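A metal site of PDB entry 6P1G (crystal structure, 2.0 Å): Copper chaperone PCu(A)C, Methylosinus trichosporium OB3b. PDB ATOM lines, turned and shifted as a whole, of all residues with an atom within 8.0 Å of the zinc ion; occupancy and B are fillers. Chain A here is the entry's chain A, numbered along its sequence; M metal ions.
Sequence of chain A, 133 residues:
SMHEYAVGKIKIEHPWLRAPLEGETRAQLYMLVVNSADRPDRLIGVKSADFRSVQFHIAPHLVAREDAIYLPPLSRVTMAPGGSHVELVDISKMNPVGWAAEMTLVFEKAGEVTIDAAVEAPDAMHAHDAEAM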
ATOM      1  N   ARG A  26      12.211 -11.124  23.808  1.00  0.00           N
ATOM      2  CA  ARG A  26      13.163 -10.119  24.264  1.00  0.00           C
ATOM      3  C   ARG A  26      14.558 -10.356  23.688  1.00  0.00           C
ATOM      4  O   ARG A  26      15.002 -11.498  23.578  1.00  0.00           O
ATOM      5  CB  ARG A  26      13.239 -10.118  25.797  1.00  0.00           C
ATOM      6  CG  ARG A  26      11.946  -9.689  26.475  1.00  0.00           C
ATOM      7  CD  ARG A  26      12.158  -9.450  27.963  1.00  0.00           C
ATOM      8  NE  ARG A  26      11.023  -8.756  28.557  1.00  0.00           N
ATOM      9  CZ  ARG A  26      11.128  -7.844  29.526  1.00  0.00           C
ATOM     10  NH1 ARG A  26      12.326  -7.514  29.990  1.00  0.00           N
ATOM     11  NH2 ARG A  26      10.044  -7.256  30.009  1.00  0.00           N
ATOM     12  N   ALA A  27      15.245  -9.276  23.334  1.00  0.00           N
ATOM     13  CA  ALA A  27      16.628  -9.354  22.874  1.00  0.00           C
ATOM     14  C   ALA A  27      17.478  -8.238  23.480  1.00  0.00           C
ATOM     15  O   ALA A  27      16.953  -7.323  24.104  1.00  0.00           O
ATOM     16  CB  ALA A  27      16.685  -9.303  21.361  1.00  0.00           C
ATOM     17  N   GLN A  28      18.784  -8.326  23.283  1.00  0.00           N
ATOM     18  CA  GLN A  28      19.710  -7.331  23.830  1.00  0.00           C
ATOM     19  C   GLN A  28      20.454  -6.625  22.709  1.00  0.00           C
ATOM     20  O   GLN A  28      21.059  -7.273  21.862  1.00  0.00           O
ATOM     21  CB  GLN A  28      20.709  -7.981  24.792  1.00  0.00           C
ATOM     22  CG  GLN A  28      20.087  -8.619  26.030  1.00  0.00           C
ATOM     23  CD  GLN A  28      19.458  -9.962  25.738  1.00  0.00           C
ATOM     24  OE1 GLN A  28      20.035 -10.806  25.046  1.00  0.00           O
ATOM     25  NE2 GLN A  28      18.258 -10.181  26.260  1.00  0.00           N
ATOM     26  N   LEU A  29      20.433  -5.301  22.721  1.00  0.00           N
ATOM     27  CA  LEU A  29      21.128  -4.502  21.714  1.00  0.00           C
ATOM     28  C   LEU A  29      22.443  -3.968  22.253  1.00  0.00           C
ATOM     29  O   LEU A  29      22.492  -3.356  23.318  1.00  0.00           O
ATOM     30  CB  LEU A  29      20.238  -3.353  21.236  1.00  0.00           C
ATOM     31  CG  LEU A  29      20.902  -2.287  20.361  1.00  0.00           C
ATOM     32  CD1 LEU A  29      21.444  -2.890  19.070  1.00  0.00           C
ATOM     33  CD2 LEU A  29      19.900  -1.185  20.056  1.00  0.00           C
ATOM     34  N   TYR A  30      23.513  -4.212  21.503  1.00  0.00           N
ATOM     35  CA  TYR A  30      24.861  -3.784  21.866  1.00  0.00           C
ATOM     36  C   TYR A  30      25.449  -2.881  20.789  1.00  0.00           C
ATOM     37  O   TYR A  30      25.051  -2.951  19.619  1.00  0.00           O
ATOM     38  CB  TYR A  30      25.769  -4.996  22.072  1.00  0.00           C
ATOM     39  CG  TYR A  30      25.221  -6.006  23.047  1.00  0.00           C
ATOM     40  CD1 TYR A  30      25.175  -5.731  24.411  1.00  0.00           C
ATOM     41  CD2 TYR A  30      24.742  -7.235  22.620  1.00  0.00           C
ATOM     42  CE1 TYR A  30      24.670  -6.659  25.309  1.00  0.00           C
ATOM     43  CE2 TYR A  30      24.236  -8.158  23.505  1.00  0.00           C
ATOM     44  CZ  TYR A  30      24.209  -7.868  24.849  1.00  0.00           C
ATOM     45  OH  TYR A  30      23.699  -8.808  25.729  1.00  0.00           O
ATOM     46  N   GLN A  55      13.873  -1.239  27.087  1.00  0.00           N
ATOM     47  CA  GLN A  55      14.311  -0.889  28.422  1.00  0.00           C
ATOM     48  C   GLN A  55      15.822  -0.774  28.430  1.00  0.00           C
ATOM     49  O   GLN A  55      16.502  -1.427  27.629  1.00  0.00           O
ATOM     50  CB  GLN A  55      13.844  -1.932  29.449  1.00  0.00           C
ATOM     51  CG  GLN A  55      12.333  -2.056  29.551  1.00  0.00           C
ATOM     52  CD  GLN A  55      11.897  -3.298  30.304  1.00  0.00           C
ATOM     53  OE1 GLN A  55      12.724  -4.072  30.782  1.00  0.00           O
ATOM     54  NE2 GLN A  55      10.587  -3.491  30.414  1.00  0.00           N
ATOM     55  N   PHE A  56      16.360   0.048  29.321  1.00  0.00           N
ATOM     56  CA  PHE A  56      17.802   0.197  29.425  1.00  0.00           C
ATOM     57  C   PHE A  56      18.283  -0.595  30.640  1.00  0.00           C
ATOM     58  O   PHE A  56      17.883  -0.330  31.774  1.00  0.00           O
ATOM     59  CB  PHE A  56      18.186   1.668  29.526  1.00  0.00           C
ATOM     60  CG  PHE A  56      17.821   2.466  28.296  1.00  0.00           C
ATOM     61  CD1 PHE A  56      16.541   2.992  28.146  1.00  0.00           C
ATOM     62  CD2 PHE A  56      18.739   2.677  27.285  1.00  0.00           C
ATOM     63  CE1 PHE A  56      16.203   3.720  27.024  1.00  0.00           C
ATOM     64  CE2 PHE A  56      18.408   3.398  26.160  1.00  0.00           C
ATOM     65  CZ  PHE A  56      17.135   3.927  26.018  1.00  0.00           C
ATOM     66  N   HIS A  57      19.143  -1.567  30.377  1.00  0.00           N
ATOM     67  CA  HIS A  57      19.599  -2.513  31.386  1.00  0.00           C
ATOM     68  C   HIS A  57      21.069  -2.439  31.800  1.00  0.00           C
ATOM     69  O   HIS A  57      21.944  -2.156  30.985  1.00  0.00           O
ATOM     70  CB  HIS A  57      19.321  -3.948  30.936  1.00  0.00           C
ATOM     71  CG  HIS A  57      17.868  -4.329  30.973  1.00  0.00           C
ATOM     72  ND1 HIS A  57      17.420  -5.570  30.606  1.00  0.00           N
ATOM     73  CD2 HIS A  57      16.775  -3.618  31.341  1.00  0.00           C
ATOM     74  CE1 HIS A  57      16.104  -5.619  30.750  1.00  0.00           C
ATOM     75  NE2 HIS A  57      15.695  -4.451  31.195  1.00  0.00           N
ATOM     76  N   ILE A  58      21.300  -2.659  33.085  1.00  0.00           N
ATOM     77  CA  ILE A  58      22.632  -2.916  33.604  1.00  0.00           C
ATOM     78  C   ILE A  58      22.720  -4.437  33.765  1.00  0.00           C
ATOM     79  O   ILE A  58      21.741  -5.066  34.132  1.00  0.00           O
ATOM     80  CB  ILE A  58      22.895  -2.209  34.956  1.00  0.00           C
ATOM     81  CG1 ILE A  58      22.620  -0.708  34.846  1.00  0.00           C
ATOM     82  CG2 ILE A  58      24.319  -2.441  35.432  1.00  0.00           C
ATOM     83  CD1 ILE A  58      23.478  -0.006  33.820  1.00  0.00           C
ATOM     84  N   ALA A  59      23.883  -5.009  33.479  1.00  0.00           N
ATOM     85  CA  ALA A  59      24.047  -6.462  33.569  1.00  0.00           C
ATOM     86  C   ALA A  59      23.787  -6.965  34.989  1.00  0.00           C
ATOM     87  O   ALA A  59      24.251  -6.379  35.955  1.00  0.00           O
ATOM     88  CB  ALA A  59      25.435  -6.859  33.121  1.00  0.00           C
ATOM     89  N   PRO A  60      23.033  -8.079  35.115  1.00  0.00           N
ATOM     90  CA  PRO A  60      22.467  -8.923  34.055  1.00  0.00           C
ATOM     91  C   PRO A  60      21.323  -8.268  33.274  1.00  0.00           C
ATOM     92  O   PRO A  60      21.494  -7.981  32.080  1.00  0.00           O
ATOM     93  CB  PRO A  60      21.946 -10.151  34.817  1.00  0.00           C
ATOM     94  CG  PRO A  60      22.608 -10.091  36.164  1.00  0.00           C
ATOM     95  CD  PRO A  60      22.777  -8.643  36.446  1.00  0.00           C
ATOM     96  N   HIS A  61      20.182  -8.043  33.914  1.00  0.00           N
ATOM     97  CA  HIS A  61      19.057  -7.398  33.255  1.00  0.00           C
ATOM     98  C   HIS A  61      18.324  -6.474  34.230  1.00  0.00           C
ATOM     99  O   HIS A  61      17.100  -6.472  34.310  1.00  0.00           O
ATOM    100  CB  HIS A  61      18.089  -8.437  32.677  1.00  0.00           C
ATOM    101  CG  HIS A  61      18.721  -9.343  31.671  1.00  0.00           C
ATOM    102  ND1 HIS A  61      18.959  -8.952  30.374  1.00  0.00           N
ATOM    103  CD2 HIS A  61      19.171 -10.613  31.773  1.00  0.00           C
ATOM    104  CE1 HIS A  61      19.532  -9.952  29.714  1.00  0.00           C
ATOM    105  NE2 HIS A  61      19.668 -10.972  30.541  1.00  0.00           N
ATOM    106  N   LEU A  62      19.106  -5.680  34.948  1.00  0.00           N
ATOM    107  CA  LEU A  62      18.584  -4.742  35.934  1.00  0.00           C
ATOM    108  C   LEU A  62      18.291  -3.377  35.314  1.00  0.00           C
ATOM    109  O   LEU A  62      19.147  -2.781  34.660  1.00  0.00           O
ATOM    110  CB  LEU A  62      19.583  -4.587  37.084  1.00  0.00           C
ATOM    111  CG  LEU A  62      19.365  -3.457  38.106  1.00  0.00           C
ATOM    112  CD1 LEU A  62      18.038  -3.624  38.845  1.00  0.00           C
ATOM    113  CD2 LEU A  62      20.526  -3.399  39.079  1.00  0.00           C
ATOM    114  N   VAL A  63      17.072  -2.888  35.527  1.00  0.00           N
ATOM    115  CA  VAL A  63      16.670  -1.568  35.050  1.00  0.00           C
ATOM    116  C   VAL A  63      17.610  -0.509  35.617  1.00  0.00           C
ATOM    117  O   VAL A  63      17.869  -0.466  36.829  1.00  0.00           O
ATOM    118  CB  VAL A  63      15.213  -1.241  35.432  1.00  0.00           C
ATOM    119  CG1 VAL A  63      14.864   0.202  35.095  1.00  0.00           C
ATOM    120  CG2 VAL A  63      14.260  -2.199  34.721  1.00  0.00           C
ATOM    121  N   SER A  84      26.305  -2.882  30.040  1.00  0.00           N
ATOM    122  CA  SER A  84      24.981  -2.298  29.894  1.00  0.00           C
ATOM    123  C   SER A  84      24.470  -2.546  28.477  1.00  0.00           C
ATOM    124  O   SER A  84      25.263  -2.767  27.557  1.00  0.00           O
ATOM    125  CB  SER A  84      24.992  -0.806  30.221  1.00  0.00           C
ATOM    126  OG  SER A  84      25.486  -0.049  29.124  1.00  0.00           O
ATOM    127  N   HIS A  85      23.161  -2.512  28.309  1.00  0.00           N
ATOM    128  CA  HIS A  85      22.566  -2.763  27.000  1.00  0.00           C
ATOM    129  C   HIS A  85      21.133  -2.257  26.942  1.00  0.00           C
ATOM    130  O   HIS A  85      20.530  -1.956  27.974  1.00  0.00           O
ATOM    131  CB  HIS A  85      22.585  -4.256  26.676  1.00  0.00           C
ATOM    132  CG  HIS A  85      21.850  -5.102  27.665  1.00  0.00           C
ATOM    133  ND1 HIS A  85      22.434  -5.578  28.822  1.00  0.00           N
ATOM    134  CD2 HIS A  85      20.564  -5.533  27.692  1.00  0.00           C
ATOM    135  CE1 HIS A  85      21.542  -6.285  29.504  1.00  0.00           C
ATOM    136  NE2 HIS A  85      20.400  -6.275  28.837  1.00  0.00           N
ATOM    137  N   VAL A  86      20.603  -2.170  25.730  1.00  0.00           N
ATOM    138  CA  VAL A  86      19.200  -1.888  25.539  1.00  0.00           C
ATOM    139  C   VAL A  86      18.443  -3.191  25.361  1.00  0.00           C
ATOM    140  O   VAL A  86      18.804  -4.018  24.519  1.00  0.00           O
ATOM    141  CB  VAL A  86      18.961  -0.968  24.324  1.00  0.00           C
ATOM    142  CG1 VAL A  86      17.466  -0.796  24.072  1.00  0.00           C
ATOM    143  CG2 VAL A  86      19.636   0.375  24.528  1.00  0.00           C
ATOM    144  N   GLU A  87      17.405  -3.393  26.159  1.00  0.00           N
ATOM    145  CA  GLU A  87      16.564  -4.564  26.031  1.00  0.00           C
ATOM    146  C   GLU A  87      15.446  -4.280  25.038  1.00  0.00           C
ATOM    147  O   GLU A  87      14.683  -3.334  25.218  1.00  0.00           O
ATOM    148  CB  GLU A  87      15.980  -4.966  27.396  1.00  0.00           C
ATOM    149  CG  GLU A  87      15.361  -6.349  27.427  1.00  0.00           C
ATOM    150  CD  GLU A  87      16.388  -7.459  27.582  1.00  0.00           C
ATOM    151  OE1 GLU A  87      17.552  -7.156  27.937  1.00  0.00           O
ATOM    152  OE2 GLU A  87      16.041  -8.637  27.364  1.00  0.00           O
ATOM    153  N   LEU A  88      15.353  -5.100  24.000  1.00  0.00           N
ATOM    154  CA  LEU A  88      14.288  -4.945  23.009  1.00  0.00           C
ATOM    155  C   LEU A  88      13.092  -5.782  23.436  1.00  0.00           C
ATOM    156  O   LEU A  88      13.184  -7.011  23.506  1.00  0.00           O
ATOM    157  CB  LEU A  88      14.784  -5.370  21.627  1.00  0.00           C
ATOM    158  CG  LEU A  88      16.095  -4.730  21.163  1.00  0.00           C
ATOM    159  CD1 LEU A  88      16.485  -5.219  19.782  1.00  0.00           C
ATOM    160  CD2 LEU A  88      15.999  -3.214  21.182  1.00  0.00           C
HETATM  161 ZN    ZN M   1      18.589  -6.994  29.558  1.00  0.00          ZN
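The zinc ion is bound by OE1 of Glu 87 (1.9 Å), NE2 of His 85 (2.1 Å), ND1 of His 57 (2.1 Å) and ND1 of His 61 (2.2 Å).
Pro 60 touches the zinc ion (O to ZN, 3.97 Å). Within 4 Å of the zinc ion: His 57, Pro 60, His 61, His 85 and Glu 87. The nearest printed residue that does not touch the zinc ion is Gln 28 (4.2 Å).
The backbone NH (N) of Glu 87 sits at hydrogen-bond distance from the backbone carbonyl oxygen (O) of Gln 55 (2.6 Å). OE1 of Gln 55 sits at hydrogen-bond distance from NE2 of His 57, 3.0 Å away. The side-chain carboxylate (OE2) of Glu 87 is in hydrogen-bond range of the side-chain amide nitrogen (NE2) of Gln 28 (2.9 Å).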
